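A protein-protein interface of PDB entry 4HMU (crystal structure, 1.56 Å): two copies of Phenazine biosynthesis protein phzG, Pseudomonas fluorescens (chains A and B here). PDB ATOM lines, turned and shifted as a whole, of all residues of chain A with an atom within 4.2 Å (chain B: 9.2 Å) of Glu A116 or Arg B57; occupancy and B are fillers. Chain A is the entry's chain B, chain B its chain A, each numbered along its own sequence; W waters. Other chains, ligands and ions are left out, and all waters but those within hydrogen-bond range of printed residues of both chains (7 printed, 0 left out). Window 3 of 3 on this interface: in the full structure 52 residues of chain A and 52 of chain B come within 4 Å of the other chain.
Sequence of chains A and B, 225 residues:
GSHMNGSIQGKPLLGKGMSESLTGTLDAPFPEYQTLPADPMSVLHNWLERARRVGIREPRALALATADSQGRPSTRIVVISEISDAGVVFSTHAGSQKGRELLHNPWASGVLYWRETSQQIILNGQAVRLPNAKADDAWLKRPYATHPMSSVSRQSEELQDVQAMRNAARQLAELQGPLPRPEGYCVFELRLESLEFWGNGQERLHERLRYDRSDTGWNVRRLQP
NE of Arg B115 sits at hydrogen-bond distance from O of Arg A57, at 2.8 Å. OE2 of Glu B58 sits at hydrogen-bond distance from OG1 of Thr A23. The side-chain hydroxyl (OG1) of Thr A23 lies within hydrogen-bond range of the guanidinium group (NE) of Arg B57 (2.8 Å). The guanidinium group of Arg A115 lies close to the guanidinium group of Arg B115 (3.3 Å). The backbone carbonyl oxygen (O) of Glu B58 lies within hydrogen-bond range of the guanidinium group (NH2) of Arg A115 (3.0 Å). The guanidinium group of Arg A115 sits at hydrogen-bond distance from the backbone carbonyl oxygen of Arg B57 (2.8 Å).
N of Leu B26 is in hydrogen-bond range of O of Glu B116. The side-chain carboxylate (OE2) of Glu B116 sits at hydrogen-bond distance from the backbone NH (N) of Arg B57, at 2.8 Å. The backbone carbonyl oxygen of Glu A116 sits at hydrogen-bond distance from the backbone NH of Leu A26. O of Arg A115 lies close to N of Gly A24 (3.3 Å). The backbone NH (N) of Thr A25 is in hydrogen-bond range of the backbone carbonyl oxygen (O) of Glu A116, at 3.1 Å. OE2 of Glu A116 is in hydrogen-bond range of N of Arg A57 (2.8 Å).
Among the printed residues, pairs that only touch across the chains: Gly A24 with Arg B57 (3.8 Å), Arg A57 with Glu B116 (3.9 Å), Arg A115 with Ala B61 (3.96 Å), Arg A115 with Tyr B113 (3.7 Å) and Glu A116 with Arg B57 (3.6 Å).
Of chain B, only Arg B57 (3.8 Å) comes within 4 Å of Gly A24. No residue of chain B comes within 4 Å of Ile A56. Of the printed residues of chain B, Arg A57 touches Arg B115 and Glu B116. Of chain B, only Arg B57 (2.8 Å), Glu B58 (3.0 Å), Ala B61 (3.96 Å), Tyr B113 (3.7 Å) and Arg B115 (3.3 Å) come within 4 Å of Arg A115. Glu A116 touches just one residue of chain B: Arg B57. No residue of chain B comes within 4 Å of Thr A117. Arg B57 touches just these residues of chain A: Thr A23, Gly A24, Arg A115 and Glu A116. Pro B59 touches none of the printed residues of chain A. Printed residues of chain A within 4 Å of Arg B115: Arg A57 and Arg A115. The nearest residue of chain B that does not touch Glu A116 is Glu B58 (6.1 Å).
Of the 18 printed residues of chain B, 6 touch a printed residue of chain A. Among the printed residues, 11 pairs touch across the chains.
Arg A57 touches Arg B115, and with the chains exchanged Arg A115 touches Arg B57. Arg A57 touches Glu B116, and with the chains exchanged Glu A116 touches Arg B57. Arg A115 touches its own counterpart, Arg B115. Of the 11 pairs that touch across the chains among the printed residues, 5 have their exchanged pair printed and touching as well.
Water W1 lies within hydrogen-bond range of OE1 of Glu B116, O of Arg B57 and NE of Arg A115. Water W7 lies within hydrogen-bond range of the backbone carbonyl oxygen (O) of Arg A115 (2.7 Å), the side-chain hydroxyl (OG) of Ser A118 (2.7 Å), the backbone NH (N) of Gly A24 (3.0 Å), the side-chain carboxylate (OE2) of Glu B58 (3.1 Å) and the backbone NH (N) of Thr A23 (3.4 Å). Water W6 lies within hydrogen-bond range of the backbone carbonyl oxygen of Tyr B113 (2.7 Å), the guanidinium group of Arg A115 (2.9 Å) and the guanidinium group of Arg B115 (3.3 Å). Water W2 lies within hydrogen-bond range of the side-chain carboxylate (OE1) of Glu A116, the backbone carbonyl oxygen (O) of Arg A57 and the guanidinium group (NE) of Arg B115. Water W3 lies within hydrogen-bond range of the backbone carbonyl oxygen (O) of Ala B61 (2.8 Å), the backbone carbonyl oxygen (O) of Pro B59 (3.2 Å), the guanidinium group (NH2) of Arg A115 (3.2 Å) and the backbone NH (N) of Tyr B113 (3.4 Å). Water W5 lies within hydrogen-bond range of the backbone NH (N) of Arg A115 (3.0 Å) and the guanidinium group (NH1) of Arg B115 (3.4 Å).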
ATOM      1  N   THR A  23     -28.001 -26.299  18.451  1.00  0.00           N
ATOM      2  CA  THR A  23     -27.568 -24.949  18.751  1.00  0.00           C
ATOM      3  C   THR A  23     -28.113 -23.910  17.768  1.00  0.00           C
ATOM      4  O   THR A  23     -27.887 -22.727  17.944  1.00  0.00           O
ATOM      5  CB  THR A  23     -26.033 -24.850  18.740  1.00  0.00           C
ATOM      6  OG1 THR A  23     -25.542 -25.144  17.427  1.00  0.00           O
ATOM      7  CG2 THR A  23     -25.416 -25.824  19.734  1.00  0.00           C
ATOM      8  N   GLY A  24     -28.820 -24.337  16.729  1.00  0.00           N
ATOM      9  CA  GLY A  24     -29.261 -23.407  15.699  1.00  0.00           C
ATOM     10  C   GLY A  24     -30.185 -22.322  16.225  1.00  0.00           C
ATOM     11  O   GLY A  24     -31.079 -22.595  17.024  1.00  0.00           O
ATOM     12  N   THR A  25     -29.971 -21.084  15.787  1.00  0.00           N
ATOM     13  CA  THR A  25     -30.844 -19.980  16.177  1.00  0.00           C
ATOM     14  C   THR A  25     -31.343 -19.119  15.024  1.00  0.00           C
ATOM     15  O   THR A  25     -32.098 -18.171  15.244  1.00  0.00           O
ATOM     16  CB  THR A  25     -30.151 -19.038  17.181  1.00  0.00           C
ATOM     17  OG1 THR A  25     -29.057 -18.364  16.538  1.00  0.00           O
ATOM     18  CG2 THR A  25     -29.663 -19.803  18.385  1.00  0.00           C
ATOM     19  N   LEU A  26     -30.924 -19.429  13.802  1.00  0.00           N
ATOM     20  CA  LEU A  26     -31.335 -18.652  12.655  1.00  0.00           C
ATOM     21  C   LEU A  26     -32.693 -19.142  12.154  1.00  0.00           C
ATOM     22  O   LEU A  26     -32.924 -20.345  12.058  1.00  0.00           O
ATOM     23  CB  LEU A  26     -30.291 -18.793  11.553  1.00  0.00           C
ATOM     24  CG  LEU A  26     -30.246 -17.755  10.445  1.00  0.00           C
ATOM     25  CD1 LEU A  26     -29.974 -16.368  11.006  1.00  0.00           C
ATOM     26  CD2 LEU A  26     -29.171 -18.148   9.455  1.00  0.00           C
ATOM     27  N   ILE A  56     -24.439 -19.657   5.803  1.00  0.00           N
ATOM     28  CA  ILE A  56     -24.154 -20.951   6.403  1.00  0.00           C
ATOM     29  C   ILE A  56     -22.721 -21.353   6.066  1.00  0.00           C
ATOM     30  O   ILE A  56     -22.271 -21.182   4.932  1.00  0.00           O
ATOM     31  CB  ILE A  56     -25.115 -22.031   5.870  1.00  0.00           C
ATOM     32  CG1 ILE A  56     -26.562 -21.694   6.235  1.00  0.00           C
ATOM     33  CG2 ILE A  56     -24.711 -23.424   6.372  1.00  0.00           C
ATOM     34  CD1 ILE A  56     -26.814 -21.585   7.702  1.00  0.00           C
ATOM     35  N   ARG A  57     -21.997 -21.883   7.043  1.00  0.00           N
ATOM     36  CA  ARG A  57     -20.633 -22.325   6.794  1.00  0.00           C
ATOM     37  C   ARG A  57     -20.599 -23.692   6.107  1.00  0.00           C
ATOM     38  O   ARG A  57     -21.115 -24.672   6.634  1.00  0.00           O
ATOM     39  CB  ARG A  57     -19.817 -22.362   8.089  1.00  0.00           C
ATOM     40  CG  ARG A  57     -18.378 -22.754   7.819  1.00  0.00           C
ATOM     41  CD  ARG A  57     -17.462 -22.467   8.959  1.00  0.00           C
ATOM     42  NE  ARG A  57     -16.072 -22.639   8.546  1.00  0.00           N
ATOM     43  CZ  ARG A  57     -15.031 -22.385   9.325  1.00  0.00           C
ATOM     44  NH1 ARG A  57     -15.224 -21.948  10.564  1.00  0.00           N
ATOM     45  NH2 ARG A  57     -13.807 -22.567   8.859  1.00  0.00           N
ATOM     46  N   TRP A 114     -26.827 -28.377   8.667  1.00  0.00           N
ATOM     47  CA  TRP A 114     -26.489 -26.969   8.875  1.00  0.00           C
ATOM     48  C   TRP A 114     -26.833 -26.605  10.314  1.00  0.00           C
ATOM     49  O   TRP A 114     -28.006 -26.426  10.668  1.00  0.00           O
ATOM     50  CB  TRP A 114     -27.253 -26.066   7.892  1.00  0.00           C
ATOM     51  CG  TRP A 114     -27.054 -26.447   6.447  1.00  0.00           C
ATOM     52  CD1 TRP A 114     -25.986 -27.113   5.917  1.00  0.00           C
ATOM     53  CD2 TRP A 114     -27.946 -26.193   5.349  1.00  0.00           C
ATOM     54  NE1 TRP A 114     -26.161 -27.299   4.565  1.00  0.00           N
ATOM     55  CE2 TRP A 114     -27.355 -26.737   4.190  1.00  0.00           C
ATOM     56  CE3 TRP A 114     -29.195 -25.572   5.235  1.00  0.00           C
ATOM     57  CZ2 TRP A 114     -27.970 -26.689   2.938  1.00  0.00           C
ATOM     58  CZ3 TRP A 114     -29.799 -25.518   3.982  1.00  0.00           C
ATOM     59  CH2 TRP A 114     -29.183 -26.072   2.857  1.00  0.00           C
ATOM     60  N   ARG A 115     -25.797 -26.506  11.138  1.00  0.00           N
ATOM     61  CA  ARG A 115     -25.966 -26.229  12.563  1.00  0.00           C
ATOM     62  C   ARG A 115     -26.709 -24.921  12.830  1.00  0.00           C
ATOM     63  O   ARG A 115     -27.482 -24.821  13.775  1.00  0.00           O
ATOM     64  CB  ARG A 115     -24.592 -26.183  13.242  1.00  0.00           C
ATOM     65  CG  ARG A 115     -23.916 -27.541  13.372  1.00  0.00           C
ATOM     66  CD  ARG A 115     -22.399 -27.404  13.407  1.00  0.00           C
ATOM     67  NE  ARG A 115     -21.746 -28.654  13.797  1.00  0.00           N
ATOM     68  CZ  ARG A 115     -21.561 -29.700  12.996  1.00  0.00           C
ATOM     69  NH1 ARG A 115     -21.970 -29.675  11.730  1.00  0.00           N
ATOM     70  NH2 ARG A 115     -20.954 -30.780  13.464  1.00  0.00           N
ATOM     71  N   GLU A 116     -26.476 -23.913  12.000  1.00  0.00           N
ATOM     72  CA  GLU A 116     -26.989 -22.578  12.272  1.00  0.00           C
ATOM     73  C   GLU A 116     -28.510 -22.508  12.192  1.00  0.00           C
ATOM     74  O   GLU A 116     -29.130 -21.712  12.887  1.00  0.00           O
ATOM     75  CB  GLU A 116     -26.379 -21.566  11.302  1.00  0.00           C
ATOM     76  CG  GLU A 116     -24.841 -21.502  11.310  1.00  0.00           C
ATOM     77  CD  GLU A 116     -24.191 -22.327  10.201  1.00  0.00           C
ATOM     78  OE1 GLU A 116     -24.663 -23.453   9.937  1.00  0.00           O
ATOM     79  OE2 GLU A 116     -23.190 -21.856   9.611  1.00  0.00           O
ATOM     80  N   THR A 117     -29.101 -23.341  11.339  1.00  0.00           N
ATOM     81  CA  THR A 117     -30.544 -23.323  11.125  1.00  0.00           C
ATOM     82  C   THR A 117     -31.232 -24.600  11.577  1.00  0.00           C
ATOM     83  O   THR A 117     -32.451 -24.714  11.431  1.00  0.00           O
ATOM     84  CB  THR A 117     -30.889 -23.163   9.634  1.00  0.00           C
ATOM     85  OG1 THR A 117     -30.186 -24.153   8.888  1.00  0.00           O
ATOM     86  CG2 THR A 117     -30.515 -21.781   9.129  1.00  0.00           C
ATOM     87  N   SER A 118     -30.467 -25.546  12.119  1.00  0.00           N
ATOM     88  CA  SER A 118     -30.983 -26.864  12.494  1.00  0.00           C
ATOM     89  C   SER A 118     -31.737 -27.499  11.330  1.00  0.00           C
ATOM     90  O   SER A 118     -32.884 -27.905  11.481  1.00  0.00           O
ATOM     91  CB  SER A 118     -31.896 -26.779  13.727  1.00  0.00           C
ATOM     92  OG  SER A 118     -31.202 -26.213  14.832  1.00  0.00           O
ATOM     93  N   LEU B  26      -9.567 -22.339  13.563  1.00  0.00           N
ATOM     94  CA  LEU B  26      -9.017 -22.616  14.892  1.00  0.00           C
ATOM     95  C   LEU B  26      -7.809 -23.551  14.806  1.00  0.00           C
ATOM     96  O   LEU B  26      -7.675 -24.326  13.858  1.00  0.00           O
ATOM     97  CB  LEU B  26     -10.082 -23.238  15.798  1.00  0.00           C
ATOM     98  CG  LEU B  26     -11.356 -22.428  16.057  1.00  0.00           C
ATOM     99  CD1 LEU B  26     -12.308 -23.221  16.940  1.00  0.00           C
ATOM    100  CD2 LEU B  26     -11.034 -21.090  16.691  1.00  0.00           C
ATOM    101  N   ARG B  50     -10.314 -32.030  23.187  1.00  0.00           N
ATOM    102  CA  ARG B  50      -9.783 -30.828  22.549  1.00  0.00           C
ATOM    103  C   ARG B  50     -10.907 -30.054  21.870  1.00  0.00           C
ATOM    104  O   ARG B  50     -10.964 -28.827  21.945  1.00  0.00           O
ATOM    105  CB  ARG B  50      -8.707 -31.200  21.523  1.00  0.00           C
ATOM    106  CG  ARG B  50      -8.193 -30.039  20.664  1.00  0.00           C
ATOM    107  CD  ARG B  50      -7.212 -29.140  21.411  1.00  0.00           C
ATOM    108  NE  ARG B  50      -6.591 -28.157  20.522  1.00  0.00           N
ATOM    109  CZ  ARG B  50      -5.741 -27.213  20.917  1.00  0.00           C
ATOM    110  NH1 ARG B  50      -5.397 -27.106  22.193  1.00  0.00           N
ATOM    111  NH2 ARG B  50      -5.230 -26.369  20.031  1.00  0.00           N
ATOM    112  N   ALA B  51     -11.800 -30.774  21.199  1.00  0.00           N
ATOM    113  CA  ALA B  51     -12.928 -30.131  20.533  1.00  0.00           C
ATOM    114  C   ALA B  51     -13.771 -29.367  21.553  1.00  0.00           C
ATOM    115  O   ALA B  51     -14.210 -28.247  21.303  1.00  0.00           O
ATOM    116  CB  ALA B  51     -13.772 -31.167  19.801  1.00  0.00           C
ATOM    117  N   ARG B  52     -13.983 -29.971  22.717  1.00  0.00           N
ATOM    118  CA  ARG B  52     -14.767 -29.322  23.755  1.00  0.00           C
ATOM    119  C   ARG B  52     -14.045 -28.089  24.296  1.00  0.00           C
ATOM    120  O   ARG B  52     -14.666 -27.051  24.542  1.00  0.00           O
ATOM    121  CB  ARG B  52     -15.060 -30.303  24.894  1.00  0.00           C
ATOM    122  CG  ARG B  52     -16.011 -29.745  25.937  1.00  0.00           C
ATOM    123  CD  ARG B  52     -16.517 -30.832  26.871  1.00  0.00           C
ATOM    124  NE  ARG B  52     -15.458 -31.363  27.724  1.00  0.00           N
ATOM    125  CZ  ARG B  52     -15.073 -30.819  28.874  1.00  0.00           C
ATOM    126  NH1 ARG B  52     -15.650 -29.710  29.323  1.00  0.00           N
ATOM    127  NH2 ARG B  52     -14.101 -31.383  29.580  1.00  0.00           N
ATOM    128  N   VAL B  54     -11.772 -26.101  22.837  1.00  0.00           N
ATOM    129  CA  VAL B  54     -11.626 -24.991  21.900  1.00  0.00           C
ATOM    130  C   VAL B  54     -12.976 -24.440  21.458  1.00  0.00           C
ATOM    131  O   VAL B  54     -13.037 -23.359  20.889  1.00  0.00           O
ATOM    132  CB  VAL B  54     -10.785 -25.366  20.653  1.00  0.00           C
ATOM    133  CG1 VAL B  54      -9.404 -25.868  21.075  1.00  0.00           C
ATOM    134  CG2 VAL B  54     -11.505 -26.394  19.782  1.00  0.00           C
ATOM    135  N   GLY B  55     -14.047 -25.184  21.725  1.00  0.00           N
ATOM    136  CA  GLY B  55     -15.390 -24.689  21.492  1.00  0.00           C
ATOM    137  C   GLY B  55     -15.950 -25.005  20.119  1.00  0.00           C
ATOM    138  O   GLY B  55     -16.719 -24.219  19.571  1.00  0.00           O
ATOM    139  N   ILE B  56     -15.581 -26.160  19.576  1.00  0.00           N
ATOM    140  CA  ILE B  56     -16.174 -26.648  18.336  1.00  0.00           C
ATOM    141  C   ILE B  56     -17.696 -26.718  18.497  1.00  0.00           C
ATOM    142  O   ILE B  56     -18.197 -27.156  19.526  1.00  0.00           O
ATOM    143  CB  ILE B  56     -15.655 -28.060  17.985  1.00  0.00           C
ATOM    144  CG1 ILE B  56     -14.146 -28.036  17.718  1.00  0.00           C
ATOM    145  CG2 ILE B  56     -16.406 -28.628  16.787  1.00  0.00           C
ATOM    146  CD1 ILE B  56     -13.723 -27.137  16.598  1.00  0.00           C
ATOM    147  N   ARG B  57     -18.428 -26.278  17.477  1.00  0.00           N
ATOM    148  CA  ARG B  57     -19.884 -26.263  17.521  1.00  0.00           C
ATOM    149  C   ARG B  57     -20.426 -27.646  17.173  1.00  0.00           C
ATOM    150  O   ARG B  57     -20.148 -28.161  16.092  1.00  0.00           O
ATOM    151  CB  ARG B  57     -20.429 -25.220  16.539  1.00  0.00           C
ATOM    152  CG  ARG B  57     -21.932 -25.018  16.628  1.00  0.00           C
ATOM    153  CD  ARG B  57     -22.400 -23.917  15.688  1.00  0.00           C
ATOM    154  NE  ARG B  57     -23.788 -23.561  15.957  1.00  0.00           N
ATOM    155  CZ  ARG B  57     -24.390 -22.455  15.533  1.00  0.00           C
ATOM    156  NH1 ARG B  57     -23.762 -21.595  14.746  1.00  0.00           N
ATOM    157  NH2 ARG B  57     -25.644 -22.226  15.884  1.00  0.00           N
ATOM    158  N   GLU B  58     -21.198 -28.224  18.097  1.00  0.00           N
ATOM    159  CA  GLU B  58     -21.799 -29.560  17.952  1.00  0.00           C
ATOM    160  C   GLU B  58     -20.817 -30.614  17.451  1.00  0.00           C
ATOM    161  O   GLU B  58     -20.995 -31.227  16.387  1.00  0.00           O
ATOM    162  CB  GLU B  58     -23.050 -29.507  17.077  1.00  0.00           C
ATOM    163  CG  GLU B  58     -24.154 -28.656  17.666  1.00  0.00           C
ATOM    164  CD  GLU B  58     -25.430 -28.713  16.850  1.00  0.00           C
ATOM    165  OE1 GLU B  58     -25.763 -29.796  16.321  1.00  0.00           O
ATOM    166  OE2 GLU B  58     -26.099 -27.666  16.735  1.00  0.00           O
ATOM    167  N   PRO B  59     -19.771 -30.855  18.236  1.00  0.00           N
ATOM    168  CA  PRO B  59     -18.748 -31.799  17.783  1.00  0.00           C
ATOM    169  C   PRO B  59     -19.228 -33.246  17.734  1.00  0.00           C
ATOM    170  O   PRO B  59     -18.605 -34.057  17.037  1.00  0.00           O
ATOM    171  CB  PRO B  59     -17.643 -31.645  18.840  1.00  0.00           C
ATOM    172  CG  PRO B  59     -18.353 -31.160  20.060  1.00  0.00           C
ATOM    173  CD  PRO B  59     -19.465 -30.277  19.554  1.00  0.00           C
ATOM    174  N   ARG B  60     -20.306 -33.569  18.447  1.00  0.00           N
ATOM    175  CA  ARG B  60     -20.757 -34.951  18.551  1.00  0.00           C
ATOM    176  C   ARG B  60     -21.910 -35.286  17.604  1.00  0.00           C
ATOM    177  O   ARG B  60     -22.531 -36.346  17.717  1.00  0.00           O
ATOM    178  CB  ARG B  60     -21.136 -35.262  19.990  1.00  0.00           C
ATOM    179  CG  ARG B  60     -19.932 -35.304  20.904  1.00  0.00           C
ATOM    180  CD  ARG B  60     -20.342 -35.676  22.299  1.00  0.00           C
ATOM    181  NE  ARG B  60     -19.197 -36.002  23.139  1.00  0.00           N
ATOM    182  CZ  ARG B  60     -19.182 -36.989  24.027  1.00  0.00           C
ATOM    183  NH1 ARG B  60     -18.096 -37.207  24.751  1.00  0.00           N
ATOM    184  NH2 ARG B  60     -20.247 -37.764  24.198  1.00  0.00           N
ATOM    185  N   ALA B  61     -22.178 -34.384  16.663  1.00  0.00           N
ATOM    186  CA  ALA B  61     -23.163 -34.625  15.608  1.00  0.00           C
ATOM    187  C   ALA B  61     -22.572 -35.570  14.560  1.00  0.00           C
ATOM    188  O   ALA B  61     -21.746 -35.181  13.731  1.00  0.00           O
ATOM    189  CB  ALA B  61     -23.601 -33.313  14.977  1.00  0.00           C
ATOM    190  N   LEU B 112     -17.711 -37.664  11.875  1.00  0.00           N
ATOM    191  CA  LEU B 112     -17.723 -36.376  12.539  1.00  0.00           C
ATOM    192  C   LEU B 112     -16.896 -35.423  11.693  1.00  0.00           C
ATOM    193  O   LEU B 112     -15.773 -35.762  11.299  1.00  0.00           O
ATOM    194  CB  LEU B 112     -17.096 -36.481  13.929  1.00  0.00           C
ATOM    195  CG  LEU B 112     -17.760 -37.425  14.932  1.00  0.00           C
ATOM    196  CD1 LEU B 112     -16.894 -37.583  16.182  1.00  0.00           C
ATOM    197  CD2 LEU B 112     -19.149 -36.905  15.310  1.00  0.00           C
ATOM    198  N   TYR B 113     -17.432 -34.240  11.407  1.00  0.00           N
ATOM    199  CA  TYR B 113     -16.673 -33.235  10.652  1.00  0.00           C
ATOM    200  C   TYR B 113     -16.775 -31.894  11.353  1.00  0.00           C
ATOM    201  O   TYR B 113     -17.877 -31.376  11.582  1.00  0.00           O
ATOM    202  CB  TYR B 113     -17.154 -33.117   9.197  1.00  0.00           C
ATOM    203  CG  TYR B 113     -16.545 -31.939   8.462  1.00  0.00           C
ATOM    204  CD1 TYR B 113     -15.182 -31.717   8.486  1.00  0.00           C
ATOM    205  CD2 TYR B 113     -17.338 -31.032   7.771  1.00  0.00           C
ATOM    206  CE1 TYR B 113     -14.624 -30.639   7.855  1.00  0.00           C
ATOM    207  CE2 TYR B 113     -16.780 -29.947   7.121  1.00  0.00           C
ATOM    208  CZ  TYR B 113     -15.418 -29.752   7.179  1.00  0.00           C
ATOM    209  OH  TYR B 113     -14.833 -28.673   6.551  1.00  0.00           O
ATOM    210  N   TRP B 114     -15.615 -31.345  11.691  1.00  0.00           N
ATOM    211  CA  TRP B 114     -15.509 -30.103  12.422  1.00  0.00           C
ATOM    212  C   TRP B 114     -14.944 -29.041  11.485  1.00  0.00           C
ATOM    213  O   TRP B 114     -13.737 -29.013  11.213  1.00  0.00           O
ATOM    214  CB  TRP B 114     -14.592 -30.299  13.640  1.00  0.00           C
ATOM    215  CG  TRP B 114     -15.050 -31.391  14.560  1.00  0.00           C
ATOM    216  CD1 TRP B 114     -16.319 -31.873  14.689  1.00  0.00           C
ATOM    217  CD2 TRP B 114     -14.241 -32.146  15.474  1.00  0.00           C
ATOM    218  NE1 TRP B 114     -16.352 -32.877  15.620  1.00  0.00           N
ATOM    219  CE2 TRP B 114     -15.090 -33.057  16.126  1.00  0.00           C
ATOM    220  CE3 TRP B 114     -12.881 -32.135  15.803  1.00  0.00           C
ATOM    221  CZ2 TRP B 114     -14.627 -33.952  17.084  1.00  0.00           C
ATOM    222  CZ3 TRP B 114     -12.428 -33.023  16.759  1.00  0.00           C
ATOM    223  CH2 TRP B 114     -13.293 -33.918  17.384  1.00  0.00           C
ATOM    224  N   ARG B 115     -15.831 -28.193  10.970  1.00  0.00           N
ATOM    225  CA  ARG B 115     -15.448 -27.137  10.036  1.00  0.00           C
ATOM    226  C   ARG B 115     -14.358 -26.225  10.584  1.00  0.00           C
ATOM    227  O   ARG B 115     -13.466 -25.802   9.844  1.00  0.00           O
ATOM    228  CB  ARG B 115     -16.665 -26.283   9.676  1.00  0.00           C
ATOM    229  CG  ARG B 115     -17.672 -26.987   8.780  1.00  0.00           C
ATOM    230  CD  ARG B 115     -19.073 -26.457   8.996  1.00  0.00           C
ATOM    231  NE  ARG B 115     -20.019 -26.930   7.981  1.00  0.00           N
ATOM    232  CZ  ARG B 115     -20.600 -28.124   7.969  1.00  0.00           C
ATOM    233  NH1 ARG B 115     -20.347 -29.016   8.916  1.00  0.00           N
ATOM    234  NH2 ARG B 115     -21.441 -28.432   6.989  1.00  0.00           N
ATOM    235  N   GLU B 116     -14.431 -25.916  11.873  1.00  0.00           N
ATOM    236  CA  GLU B 116     -13.565 -24.888  12.456  1.00  0.00           C
ATOM    237  C   GLU B 116     -12.098 -25.274  12.433  1.00  0.00           C
ATOM    238  O   GLU B 116     -11.236 -24.401  12.330  1.00  0.00           O
ATOM    239  CB  GLU B 116     -13.957 -24.589  13.904  1.00  0.00           C
ATOM    240  CG  GLU B 116     -15.371 -24.105  14.096  1.00  0.00           C
ATOM    241  CD  GLU B 116     -16.313 -25.215  14.499  1.00  0.00           C
ATOM    242  OE1 GLU B 116     -16.226 -26.323  13.925  1.00  0.00           O
ATOM    243  OE2 GLU B 116     -17.140 -24.979  15.401  1.00  0.00           O
ATOM    244  N   THR B 117     -11.819 -26.571  12.549  1.00  0.00           N
ATOM    245  CA  THR B 117     -10.443 -27.078  12.573  1.00  0.00           C
ATOM    246  C   THR B 117     -10.099 -27.906  11.337  1.00  0.00           C
ATOM    247  O   THR B 117      -9.001 -28.452  11.245  1.00  0.00           O
ATOM    248  CB  THR B 117     -10.215 -27.970  13.786  1.00  0.00           C
ATOM    249  OG1 THR B 117     -11.224 -28.990  13.808  1.00  0.00           O
ATOM    250  CG2 THR B 117     -10.276 -27.153  15.062  1.00  0.00           C
HETATM  251  O   HOH W   1     -18.648 -27.463  13.855  1.00  0.00           O
HETATM  252  O   HOH W   2     -22.599 -25.014   9.026  1.00  0.00           O
HETATM  253  O   HOH W   3     -19.466 -33.518  14.039  1.00  0.00           O
HETATM  254  O   HOH W   4     -18.660 -28.747  11.444  1.00  0.00           O
HETATM  255  O   HOH W   5     -23.187 -27.456  10.089  1.00  0.00           O
HETATM  256  O   HOH W   6     -20.356 -31.822  10.590  1.00  0.00           O
HETATM  257  O   HOH W   7     -28.603 -26.851  15.115  1.00  0.00           O
